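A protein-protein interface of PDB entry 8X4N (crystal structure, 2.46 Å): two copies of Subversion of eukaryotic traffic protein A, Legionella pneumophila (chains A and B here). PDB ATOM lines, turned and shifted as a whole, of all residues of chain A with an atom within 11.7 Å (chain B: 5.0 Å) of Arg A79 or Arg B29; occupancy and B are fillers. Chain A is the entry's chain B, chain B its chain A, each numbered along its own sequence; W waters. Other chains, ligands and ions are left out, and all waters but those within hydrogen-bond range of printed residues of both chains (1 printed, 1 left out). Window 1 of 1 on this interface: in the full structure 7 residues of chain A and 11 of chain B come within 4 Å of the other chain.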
ATOM      1  N   LEU A  24       6.666  12.914  32.322  1.00  0.00           N
ATOM      2  CA  LEU A  24       5.485  13.755  32.428  1.00  0.00           C
ATOM      3  C   LEU A  24       4.704  13.728  31.119  1.00  0.00           C
ATOM      4  O   LEU A  24       5.248  13.393  30.067  1.00  0.00           O
ATOM      5  CB  LEU A  24       5.921  15.191  32.736  1.00  0.00           C
ATOM      6  CG  LEU A  24       6.272  15.469  34.193  1.00  0.00           C
ATOM      7  CD1 LEU A  24       6.627  16.935  34.392  1.00  0.00           C
ATOM      8  CD2 LEU A  24       5.122  15.060  35.107  1.00  0.00           C
ATOM      9  N   ASN A  41       0.947  14.367  22.436  1.00  0.00           N
ATOM     10  CA  ASN A  41       0.119  15.517  22.090  1.00  0.00           C
ATOM     11  C   ASN A  41      -0.275  15.495  20.618  1.00  0.00           C
ATOM     12  O   ASN A  41      -1.452  15.648  20.296  1.00  0.00           O
ATOM     13  CB  ASN A  41       0.822  16.849  22.363  1.00  0.00           C
ATOM     14  CG  ASN A  41       1.093  17.100  23.831  1.00  0.00           C
ATOM     15  OD1 ASN A  41       0.313  16.687  24.689  1.00  0.00           O
ATOM     16  ND2 ASN A  41       2.203  17.761  24.125  1.00  0.00           N
ATOM     17  N   MET A  45      -4.046  14.964  18.878  1.00  0.00           N
ATOM     18  CA  MET A  45      -4.675  15.932  17.991  1.00  0.00           C
ATOM     19  C   MET A  45      -5.127  15.249  16.698  1.00  0.00           C
ATOM     20  O   MET A  45      -6.092  15.682  16.074  1.00  0.00           O
ATOM     21  CB  MET A  45      -3.704  17.065  17.646  1.00  0.00           C
ATOM     22  CG  MET A  45      -3.656  18.155  18.694  1.00  0.00           C
ATOM     23  SD  MET A  45      -2.507  19.498  18.263  1.00  0.00           S
ATOM     24  CE  MET A  45      -0.973  18.605  18.013  1.00  0.00           C
ATOM     25  N   LYS A  72       3.580  17.234  10.454  1.00  0.00           N
ATOM     26  CA  LYS A  72       4.701  18.028   9.974  1.00  0.00           C
ATOM     27  C   LYS A  72       5.155  19.018  11.046  1.00  0.00           C
ATOM     28  O   LYS A  72       6.353  19.211  11.227  1.00  0.00           O
ATOM     29  CB  LYS A  72       4.340  18.747   8.671  1.00  0.00           C
ATOM     30  CG  LYS A  72       4.346  17.854   7.437  1.00  0.00           C
ATOM     31  CD  LYS A  72       4.048  18.581   6.146  1.00  0.00           C
ATOM     32  CE  LYS A  72       4.088  17.665   4.941  1.00  0.00           C
ATOM     33  NZ  LYS A  72       3.885  18.420   3.683  1.00  0.00           N
ATOM     34  N   LEU A  73       4.199  19.637  11.748  1.00  0.00           N
ATOM     35  CA  LEU A  73       4.519  20.556  12.831  1.00  0.00           C
ATOM     36  C   LEU A  73       5.122  19.800  14.016  1.00  0.00           C
ATOM     37  O   LEU A  73       6.030  20.306  14.676  1.00  0.00           O
ATOM     38  CB  LEU A  73       3.261  21.325  13.253  1.00  0.00           C
ATOM     39  CG  LEU A  73       3.001  22.628  12.496  1.00  0.00           C
ATOM     40  CD1 LEU A  73       2.371  22.363  11.134  1.00  0.00           C
ATOM     41  CD2 LEU A  73       2.124  23.566  13.317  1.00  0.00           C
ATOM     42  N   SER A  74       4.613  18.594  14.294  1.00  0.00           N
ATOM     43  CA  SER A  74       5.133  17.794  15.395  1.00  0.00           C
ATOM     44  C   SER A  74       6.572  17.367  15.104  1.00  0.00           C
ATOM     45  O   SER A  74       7.402  17.316  16.009  1.00  0.00           O
ATOM     46  CB  SER A  74       4.243  16.608  15.678  1.00  0.00           C
ATOM     47  OG  SER A  74       2.996  17.030  16.204  1.00  0.00           O
ATOM     48  N   ASN A  75       6.853  17.088  13.827  1.00  0.00           N
ATOM     49  CA  ASN A  75       8.150  16.600  13.390  1.00  0.00           C
ATOM     50  C   ASN A  75       9.224  17.659  13.649  1.00  0.00           C
ATOM     51  O   ASN A  75      10.372  17.328  13.935  1.00  0.00           O
ATOM     52  CB  ASN A  75       8.106  16.213  11.908  1.00  0.00           C
ATOM     53  CG  ASN A  75       8.919  14.983  11.569  1.00  0.00           C
ATOM     54  OD1 ASN A  75       9.485  14.339  12.449  1.00  0.00           O
ATOM     55  ND2 ASN A  75       8.960  14.634  10.295  1.00  0.00           N
ATOM     56  N   GLN A  76       8.838  18.936  13.541  1.00  0.00           N
ATOM     57  CA  GLN A  76       9.763  20.047  13.689  1.00  0.00           C
ATOM     58  C   GLN A  76      10.058  20.320  15.163  1.00  0.00           C
ATOM     59  O   GLN A  76      11.133  20.812  15.493  1.00  0.00           O
ATOM     60  CB  GLN A  76       9.180  21.298  13.030  1.00  0.00           C
ATOM     61  CG  GLN A  76       9.092  21.208  11.510  1.00  0.00           C
ATOM     62  CD  GLN A  76       8.322  22.360  10.907  1.00  0.00           C
ATOM     63  OE1 GLN A  76       7.825  23.240  11.607  1.00  0.00           O
ATOM     64  NE2 GLN A  76       8.214  22.360   9.588  1.00  0.00           N
ATOM     65  N   LEU A  77       9.096  20.014  16.041  1.00  0.00           N
ATOM     66  CA  LEU A  77       9.205  20.333  17.456  1.00  0.00           C
ATOM     67  C   LEU A  77      10.138  19.340  18.150  1.00  0.00           C
ATOM     68  O   LEU A  77       9.859  18.144  18.178  1.00  0.00           O
ATOM     69  CB  LEU A  77       7.802  20.287  18.071  1.00  0.00           C
ATOM     70  CG  LEU A  77       7.691  20.789  19.509  1.00  0.00           C
ATOM     71  CD1 LEU A  77       7.560  22.304  19.547  1.00  0.00           C
ATOM     72  CD2 LEU A  77       6.522  20.130  20.228  1.00  0.00           C
ATOM     73  N   ASN A  78      11.238  19.854  18.720  1.00  0.00           N
ATOM     74  CA  ASN A  78      12.151  19.051  19.519  1.00  0.00           C
ATOM     75  C   ASN A  78      12.585  19.851  20.749  1.00  0.00           C
ATOM     76  O   ASN A  78      13.755  19.867  21.117  1.00  0.00           O
ATOM     77  CB  ASN A  78      13.336  18.548  18.686  1.00  0.00           C
ATOM     78  CG  ASN A  78      14.121  17.452  19.382  1.00  0.00           C
ATOM     79  OD1 ASN A  78      13.536  16.505  19.908  1.00  0.00           O
ATOM     80  ND2 ASN A  78      15.440  17.579  19.412  1.00  0.00           N
ATOM     81  N   ARG A  79      11.604  20.463  21.417  1.00  0.00           N
ATOM     82  CA  ARG A  79      11.832  21.337  22.554  1.00  0.00           C
ATOM     83  C   ARG A  79      11.846  20.526  23.855  1.00  0.00           C
ATOM     84  O   ARG A  79      11.961  21.087  24.945  1.00  0.00           O
ATOM     85  CB  ARG A  79      10.728  22.402  22.538  1.00  0.00           C
ATOM     86  CG  ARG A  79      10.985  23.619  23.414  1.00  0.00           C
ATOM     87  CD  ARG A  79       9.949  24.711  23.211  1.00  0.00           C
ATOM     88  NE  ARG A  79      10.100  25.407  21.939  1.00  0.00           N
ATOM     89  CZ  ARG A  79       9.177  25.456  20.981  1.00  0.00           C
ATOM     90  NH1 ARG A  79       8.054  24.769  21.092  1.00  0.00           N
ATOM     91  NH2 ARG A  79       9.391  26.188  19.902  1.00  0.00           N
ATOM     92  N   HIS A  80      11.776  19.193  23.736  1.00  0.00           N
ATOM     93  CA  HIS A  80      11.487  18.321  24.863  1.00  0.00           C
ATOM     94  C   HIS A  80      12.628  18.359  25.873  1.00  0.00           C
ATOM     95  O   HIS A  80      13.787  18.473  25.487  1.00  0.00           O
ATOM     96  CB  HIS A  80      11.217  16.892  24.380  1.00  0.00           C
ATOM     97  CG  HIS A  80      10.064  16.793  23.446  1.00  0.00           C
ATOM     98  ND1 HIS A  80      10.175  17.096  22.107  1.00  0.00           N
ATOM     99  CD2 HIS A  80       8.788  16.427  23.645  1.00  0.00           C
ATOM    100  CE1 HIS A  80       8.997  16.914  21.526  1.00  0.00           C
ATOM    101  NE2 HIS A  80       8.140  16.508  22.443  1.00  0.00           N
ATOM    102  N   THR A  81      12.272  18.252  27.163  1.00  0.00           N
ATOM    103  CA  THR A  81      13.243  18.153  28.243  1.00  0.00           C
ATOM    104  C   THR A  81      13.413  16.681  28.631  1.00  0.00           C
ATOM    105  O   THR A  81      12.735  15.806  28.093  1.00  0.00           O
ATOM    106  CB  THR A  81      12.851  19.013  29.460  1.00  0.00           C
ATOM    107  OG1 THR A  81      11.823  18.387  30.223  1.00  0.00           O
ATOM    108  CG2 THR A  81      12.368  20.395  29.091  1.00  0.00           C
ATOM    109  N   PHE A  82      14.326  16.436  29.579  1.00  0.00           N
ATOM    110  CA  PHE A  82      14.534  15.117  30.154  1.00  0.00           C
ATOM    111  C   PHE A  82      13.239  14.547  30.737  1.00  0.00           C
ATOM    112  O   PHE A  82      13.067  13.327  30.763  1.00  0.00           O
ATOM    113  CB  PHE A  82      15.589  15.178  31.262  1.00  0.00           C
ATOM    114  CG  PHE A  82      16.034  13.825  31.759  1.00  0.00           C
ATOM    115  CD1 PHE A  82      16.914  13.053  31.014  1.00  0.00           C
ATOM    116  CD2 PHE A  82      15.541  13.302  32.946  1.00  0.00           C
ATOM    117  CE1 PHE A  82      17.317  11.805  31.463  1.00  0.00           C
ATOM    118  CE2 PHE A  82      15.930  12.047  33.386  1.00  0.00           C
ATOM    119  CZ  PHE A  82      16.821  11.304  32.646  1.00  0.00           C
ATOM    120  N   PHE A  83      12.354  15.433  31.227  1.00  0.00           N
ATOM    121  CA  PHE A  83      11.174  15.047  31.988  1.00  0.00           C
ATOM    122  C   PHE A  83       9.984  14.713  31.090  1.00  0.00           C
ATOM    123  O   PHE A  83       9.010  14.157  31.594  1.00  0.00           O
ATOM    124  CB  PHE A  83      10.760  16.174  32.939  1.00  0.00           C
ATOM    125  CG  PHE A  83      11.684  16.447  34.103  1.00  0.00           C
ATOM    126  CD1 PHE A  83      12.772  15.632  34.384  1.00  0.00           C
ATOM    127  CD2 PHE A  83      11.452  17.535  34.934  1.00  0.00           C
ATOM    128  CE1 PHE A  83      13.599  15.896  35.463  1.00  0.00           C
ATOM    129  CE2 PHE A  83      12.283  17.795  36.011  1.00  0.00           C
ATOM    130  CZ  PHE A  83      13.352  16.976  36.273  1.00  0.00           C
ATOM    131  N   ASN A  84      10.049  15.086  29.796  1.00  0.00           N
ATOM    132  CA  ASN A  84       8.965  14.871  28.840  1.00  0.00           C
ATOM    133  C   ASN A  84       9.517  14.507  27.461  1.00  0.00           C
ATOM    134  O   ASN A  84       9.088  15.062  26.450  1.00  0.00           O
ATOM    135  CB  ASN A  84       8.039  16.087  28.723  1.00  0.00           C
ATOM    136  CG  ASN A  84       8.714  17.375  28.284  1.00  0.00           C
ATOM    137  OD1 ASN A  84       9.923  17.545  28.420  1.00  0.00           O
ATOM    138  ND2 ASN A  84       7.925  18.314  27.792  1.00  0.00           N
ATOM    139  N   GLN A  85      10.440  13.540  27.417  1.00  0.00           N
ATOM    140  CA  GLN A  85      11.064  13.128  26.170  1.00  0.00           C
ATOM    141  C   GLN A  85      10.040  12.465  25.248  1.00  0.00           C
ATOM    142  O   GLN A  85       9.211  11.670  25.693  1.00  0.00           O
ATOM    143  CB  GLN A  85      12.193  12.127  26.424  1.00  0.00           C
ATOM    144  CG  GLN A  85      13.380  12.697  27.181  1.00  0.00           C
ATOM    145  CD  GLN A  85      14.272  11.590  27.687  1.00  0.00           C
ATOM    146  OE1 GLN A  85      14.614  10.665  26.954  1.00  0.00           O
ATOM    147  NE2 GLN A  85      14.627  11.651  28.962  1.00  0.00           N
ATOM    148  N   ARG A  86      10.145  12.789  23.951  1.00  0.00           N
ATOM    149  CA  ARG A  86       9.462  12.054  22.900  1.00  0.00           C
ATOM    150  C   ARG A  86      10.182  10.732  22.657  1.00  0.00           C
ATOM    151  O   ARG A  86      11.394  10.710  22.449  1.00  0.00           O
ATOM    152  CB  ARG A  86       9.438  12.846  21.592  1.00  0.00           C
ATOM    153  CG  ARG A  86       8.755  12.112  20.444  1.00  0.00           C
ATOM    154  CD  ARG A  86       8.755  12.936  19.177  1.00  0.00           C
ATOM    155  NE  ARG A  86       7.988  14.154  19.350  1.00  0.00           N
ATOM    156  CZ  ARG A  86       7.996  15.173  18.503  1.00  0.00           C
ATOM    157  NH1 ARG A  86       8.791  15.142  17.450  1.00  0.00           N
ATOM    158  NH2 ARG A  86       7.206  16.213  18.712  1.00  0.00           N
ATOM    159  N   GLN A  87       9.407   9.641  22.645  1.00  0.00           N
ATOM    160  CA  GLN A  87       9.955   8.308  22.453  1.00  0.00           C
ATOM    161  C   GLN A  87      10.296   8.130  20.975  1.00  0.00           C
ATOM    162  O   GLN A  87       9.747   8.822  20.118  1.00  0.00           O
ATOM    163  CB  GLN A  87       8.959   7.262  22.957  1.00  0.00           C
ATOM    164  CG  GLN A  87       8.527   7.477  24.400  1.00  0.00           C
ATOM    165  CD  GLN A  87       9.688   7.435  25.363  1.00  0.00           C
ATOM    166  OE1 GLN A  87      10.352   6.413  25.499  1.00  0.00           O
ATOM    167  NE2 GLN A  87       9.939   8.544  26.041  1.00  0.00           N
ATOM    168  N   TYR A  94       5.502  10.238  13.469  1.00  0.00           N
ATOM    169  CA  TYR A  94       5.310  11.575  12.927  1.00  0.00           C
ATOM    170  C   TYR A  94       6.056  11.721  11.601  1.00  0.00           C
ATOM    171  O   TYR A  94       5.602  12.452  10.723  1.00  0.00           O
ATOM    172  CB  TYR A  94       5.754  12.665  13.908  1.00  0.00           C
ATOM    173  CG  TYR A  94       4.949  12.792  15.181  1.00  0.00           C
ATOM    174  CD1 TYR A  94       3.569  12.641  15.198  1.00  0.00           C
ATOM    175  CD2 TYR A  94       5.568  13.128  16.376  1.00  0.00           C
ATOM    176  CE1 TYR A  94       2.837  12.777  16.370  1.00  0.00           C
ATOM    177  CE2 TYR A  94       4.850  13.272  17.552  1.00  0.00           C
ATOM    178  CZ  TYR A  94       3.479  13.093  17.553  1.00  0.00           C
ATOM    179  OH  TYR A  94       2.771  13.227  18.725  1.00  0.00           O
ATOM    180  N   ASN B  27      18.960  22.724  28.886  1.00  0.00           N
ATOM    181  CA  ASN B  27      18.002  22.998  27.839  1.00  0.00           C
ATOM    182  C   ASN B  27      18.222  24.435  27.395  1.00  0.00           C
ATOM    183  O   ASN B  27      18.196  25.331  28.234  1.00  0.00           O
ATOM    184  CB  ASN B  27      16.572  22.801  28.336  1.00  0.00           C
ATOM    185  CG  ASN B  27      16.293  21.384  28.780  1.00  0.00           C
ATOM    186  OD1 ASN B  27      15.862  20.552  27.984  1.00  0.00           O
ATOM    187  ND2 ASN B  27      16.484  21.123  30.062  1.00  0.00           N
ATOM    188  N   THR B  28      18.462  24.615  26.089  1.00  0.00           N
ATOM    189  CA  THR B  28      18.661  25.927  25.504  1.00  0.00           C
ATOM    190  C   THR B  28      17.296  26.543  25.229  1.00  0.00           C
ATOM    191  O   THR B  28      16.418  25.888  24.668  1.00  0.00           O
ATOM    192  CB  THR B  28      19.522  25.876  24.234  1.00  0.00           C
ATOM    193  OG1 THR B  28      18.964  24.918  23.336  1.00  0.00           O
ATOM    194  CG2 THR B  28      20.960  25.507  24.518  1.00  0.00           C
ATOM    195  N   ARG B  29      17.131  27.792  25.667  1.00  0.00           N
ATOM    196  CA  ARG B  29      15.940  28.565  25.367  1.00  0.00           C
ATOM    197  C   ARG B  29      16.386  29.962  24.941  1.00  0.00           C
ATOM    198  O   ARG B  29      17.445  30.430  25.354  1.00  0.00           O
ATOM    199  CB  ARG B  29      15.015  28.558  26.588  1.00  0.00           C
ATOM    200  CG  ARG B  29      14.391  27.205  26.891  1.00  0.00           C
ATOM    201  CD  ARG B  29      13.367  26.815  25.840  1.00  0.00           C
ATOM    202  NE  ARG B  29      12.596  25.636  26.206  1.00  0.00           N
ATOM    203  CZ  ARG B  29      13.021  24.382  26.101  1.00  0.00           C
ATOM    204  NH1 ARG B  29      14.225  24.121  25.618  1.00  0.00           N
ATOM    205  NH2 ARG B  29      12.225  23.390  26.471  1.00  0.00           N
ATOM    206  N   GLN B  30      15.593  30.615  24.088  1.00  0.00           N
ATOM    207  CA  GLN B  30      15.958  31.933  23.599  1.00  0.00           C
ATOM    208  C   GLN B  30      14.970  32.961  24.141  1.00  0.00           C
ATOM    209  O   GLN B  30      13.761  32.779  24.021  1.00  0.00           O
ATOM    210  CB  GLN B  30      16.000  31.946  22.069  1.00  0.00           C
ATOM    211  CG  GLN B  30      16.949  32.996  21.512  1.00  0.00           C
ATOM    212  CD  GLN B  30      17.128  32.866  20.021  1.00  0.00           C
ATOM    213  OE1 GLN B  30      16.343  32.213  19.338  1.00  0.00           O
ATOM    214  NE2 GLN B  30      18.166  33.502  19.504  1.00  0.00           N
ATOM    215  N   LEU B  31      15.505  34.041  24.723  1.00  0.00           N
ATOM    216  CA  LEU B  31      14.696  35.161  25.185  1.00  0.00           C
ATOM    217  C   LEU B  31      14.175  35.937  23.975  1.00  0.00           C
ATOM    218  O   LEU B  31      14.620  35.711  22.851  1.00  0.00           O
ATOM    219  CB  LEU B  31      15.553  36.057  26.089  1.00  0.00           C
ATOM    220  CG  LEU B  31      16.261  35.352  27.245  1.00  0.00           C
ATOM    221  CD1 LEU B  31      16.891  36.357  28.201  1.00  0.00           C
ATOM    222  CD2 LEU B  31      15.303  34.430  27.989  1.00  0.00           C
ATOM    223  N   ARG B  35      18.807  36.605  23.246  1.00  0.00           N
ATOM    224  CA  ARG B  35      19.806  35.948  24.075  1.00  0.00           C
ATOM    225  C   ARG B  35      19.389  34.505  24.365  1.00  0.00           C
ATOM    226  O   ARG B  35      18.220  34.221  24.620  1.00  0.00           O
ATOM    227  CB  ARG B  35      19.994  36.753  25.366  1.00  0.00           C
ATOM    228  CG  ARG B  35      21.007  36.179  26.348  1.00  0.00           C
ATOM    229  CD  ARG B  35      20.877  36.870  27.691  1.00  0.00           C
ATOM    230  NE  ARG B  35      21.441  36.088  28.780  1.00  0.00           N
ATOM    231  CZ  ARG B  35      21.126  36.250  30.060  1.00  0.00           C
ATOM    232  NH1 ARG B  35      20.246  37.168  30.419  1.00  0.00           N
ATOM    233  NH2 ARG B  35      21.685  35.480  30.979  1.00  0.00           N
ATOM    234  N   VAL B  36      20.380  33.606  24.339  1.00  0.00           N
ATOM    235  CA  VAL B  36      20.174  32.188  24.575  1.00  0.00           C
ATOM    236  C   VAL B  36      20.636  31.852  25.991  1.00  0.00           C
ATOM    237  O   VAL B  36      21.737  32.218  26.398  1.00  0.00           O
ATOM    238  CB  VAL B  36      20.930  31.329  23.540  1.00  0.00           C
ATOM    239  CG1 VAL B  36      20.779  29.841  23.821  1.00  0.00           C
ATOM    240  CG2 VAL B  36      20.500  31.650  22.115  1.00  0.00           C
ATOM    241  N   ILE B  37      19.792  31.124  26.723  1.00  0.00           N
ATOM    242  CA  ILE B  37      20.149  30.637  28.046  1.00  0.00           C
ATOM    243  C   ILE B  37      20.213  29.109  28.020  1.00  0.00           C
ATOM    244  O   ILE B  37      19.674  28.464  27.122  1.00  0.00           O
ATOM    245  CB  ILE B  37      19.175  31.172  29.116  1.00  0.00           C
ATOM    246  CG1 ILE B  37      17.713  30.859  28.781  1.00  0.00           C
ATOM    247  CG2 ILE B  37      19.390  32.664  29.331  1.00  0.00           C
ATOM    248  CD1 ILE B  37      16.749  31.174  29.896  1.00  0.00           C
ATOM    249  N   ILE B  39      19.307  26.155  30.765  1.00  0.00           N
ATOM    250  CA  ILE B  39      18.643  25.990  32.052  1.00  0.00           C
ATOM    251  C   ILE B  39      18.191  24.540  32.253  1.00  0.00           C
ATOM    252  O   ILE B  39      18.002  23.798  31.290  1.00  0.00           O
ATOM    253  CB  ILE B  39      17.465  26.979  32.185  1.00  0.00           C
ATOM    254  CG1 ILE B  39      16.461  26.820  31.041  1.00  0.00           C
ATOM    255  CG2 ILE B  39      17.972  28.413  32.303  1.00  0.00           C
ATOM    256  CD1 ILE B  39      15.187  27.578  31.243  1.00  0.00           C
ATOM    257  N   ALA B  44      12.871  24.810  32.322  1.00  0.00           N
ATOM    258  CA  ALA B  44      12.634  24.894  30.886  1.00  0.00           C
ATOM    259  C   ALA B  44      11.162  24.670  30.557  1.00  0.00           C
ATOM    260  O   ALA B  44      10.654  25.271  29.619  1.00  0.00           O
ATOM    261  CB  ALA B  44      13.486  23.885  30.159  1.00  0.00           C
ATOM    262  N   PHE B  47       9.366  27.708  31.577  1.00  0.00           N
ATOM    263  CA  PHE B  47       9.590  28.702  30.539  1.00  0.00           C
ATOM    264  C   PHE B  47       8.629  28.480  29.371  1.00  0.00           C
ATOM    265  O   PHE B  47       8.146  29.439  28.781  1.00  0.00           O
ATOM    266  CB  PHE B  47      11.055  28.662  30.090  1.00  0.00           C
ATOM    267  CG  PHE B  47      11.431  29.706  29.070  1.00  0.00           C
ATOM    268  CD1 PHE B  47      11.192  29.499  27.719  1.00  0.00           C
ATOM    269  CD2 PHE B  47      11.997  30.909  29.466  1.00  0.00           C
ATOM    270  CE1 PHE B  47      11.527  30.466  26.786  1.00  0.00           C
ATOM    271  CE2 PHE B  47      12.328  31.876  28.529  1.00  0.00           C
ATOM    272  CZ  PHE B  47      12.093  31.653  27.191  1.00  0.00           C
ATOM    273  N   ASP B  48       8.342  27.217  29.049  1.00  0.00           N
ATOM    274  CA  ASP B  48       7.489  26.880  27.921  1.00  0.00           C
ATOM    275  C   ASP B  48       6.030  27.240  28.212  1.00  0.00           C
ATOM    276  O   ASP B  48       5.279  27.528  27.284  1.00  0.00           O
ATOM    277  CB  ASP B  48       7.646  25.401  27.555  1.00  0.00           C
ATOM    278  CG  ASP B  48       9.023  25.039  27.012  1.00  0.00           C
ATOM    279  OD1 ASP B  48       9.783  25.976  26.649  1.00  0.00           O
ATOM    280  OD2 ASP B  48       9.341  23.818  26.973  1.00  0.00           O
HETATM  281  O   HOH W   1       9.195  21.277  26.775  1.00  0.00           O
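The guanidinium group (NH2) of Arg B29 lies within hydrogen-bond range of the backbone carbonyl oxygen (O) of Arg A79 (2.8 Å).
The side-chain carboxylate of Asp B48 lies within salt-bridge range of the guanidinium group of Arg B29, 2.9 Å away.
The side-chain amide oxygen of Asn A84 sits at hydrogen-bond distance from the side-chain hydroxyl of Thr A81, 2.8 Å away.
The backbone carbonyl oxygen (O) of Arg B29 is in hydrogen-bond range of the backbone NH (N) of Ile B37 (2.8 Å).
The backbone NH (N) of Asn B27 lies within hydrogen-bond range of the backbone carbonyl oxygen (O) of Ile B39, 2.8 Å away.
The side-chain hydroxyl (OG1) of Thr A81 lies close to the backbone NH (N) of Phe A83 (3.2 Å).
CD of Arg A79 touches OD1 of Asp B48, at 3.7 Å.
His A80 touches Asn B27.
Thr A81 touches Asn B27.
CG2 of Thr A81 touches NH2 of Arg B29 (3.98 Å).
Thr A81 touches Ala B44.
Leu A24 touches none of the printed residues of chain B.
Asn A75 touches none of the printed residues of chain B.
Arg A79 touches just these residues of chain B: Arg B29 and Asp B48.
Printed residues of chain B within 4 Å of His A80: Asn B27 (3.9 Å).
Printed residues of chain B within 4 Å of Thr A81: Asn B27 (3.6 Å), Arg B29 (3.98 Å) and Ala B44 (3.8 Å).
Asn B27 touches just these residues of chain A: His A80 and Thr A81.
No residue of chain A comes within 4 Å of Thr B28.
Printed residues of chain A within 4 Å of Arg B29: Arg A79 (2.8 Å) and Thr A81 (3.98 Å).
No residue of chain A comes within 4 Å of Leu B31.
No residue of chain A comes within 4 Å of Val B36.
No residue of chain A comes within 4 Å of Ile B37.
No residue of chain A comes within 4 Å of Ile B39.
Of chain A, only Arg A79 comes within 4 Å of Asp B48.
The nearest printed residue of chain A that does not touch Arg B29 is His A80 (5.0 Å).
The nearest printed residue of chain B that does not touch Thr A81 is Asp B48 (5.0 Å).
Printed residues of chain A that touch a printed residue of chain B: Arg A79, His A80 and Thr A81.
Of the 12 printed residues of chain B, 4 touch a printed residue of chain A.
Hydrophobic or aromatic side chains of chain B that line the printed part of chain A: Ala B44.
No position is printed for both chains.
Of the 6 pairs that touch across the chains among the printed residues, none has its exchanged pair printed and touching as well.
Water W1 lies within hydrogen-bond range of OD2 of Asp B48, O of Arg A79 and ND2 of Asn A84.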
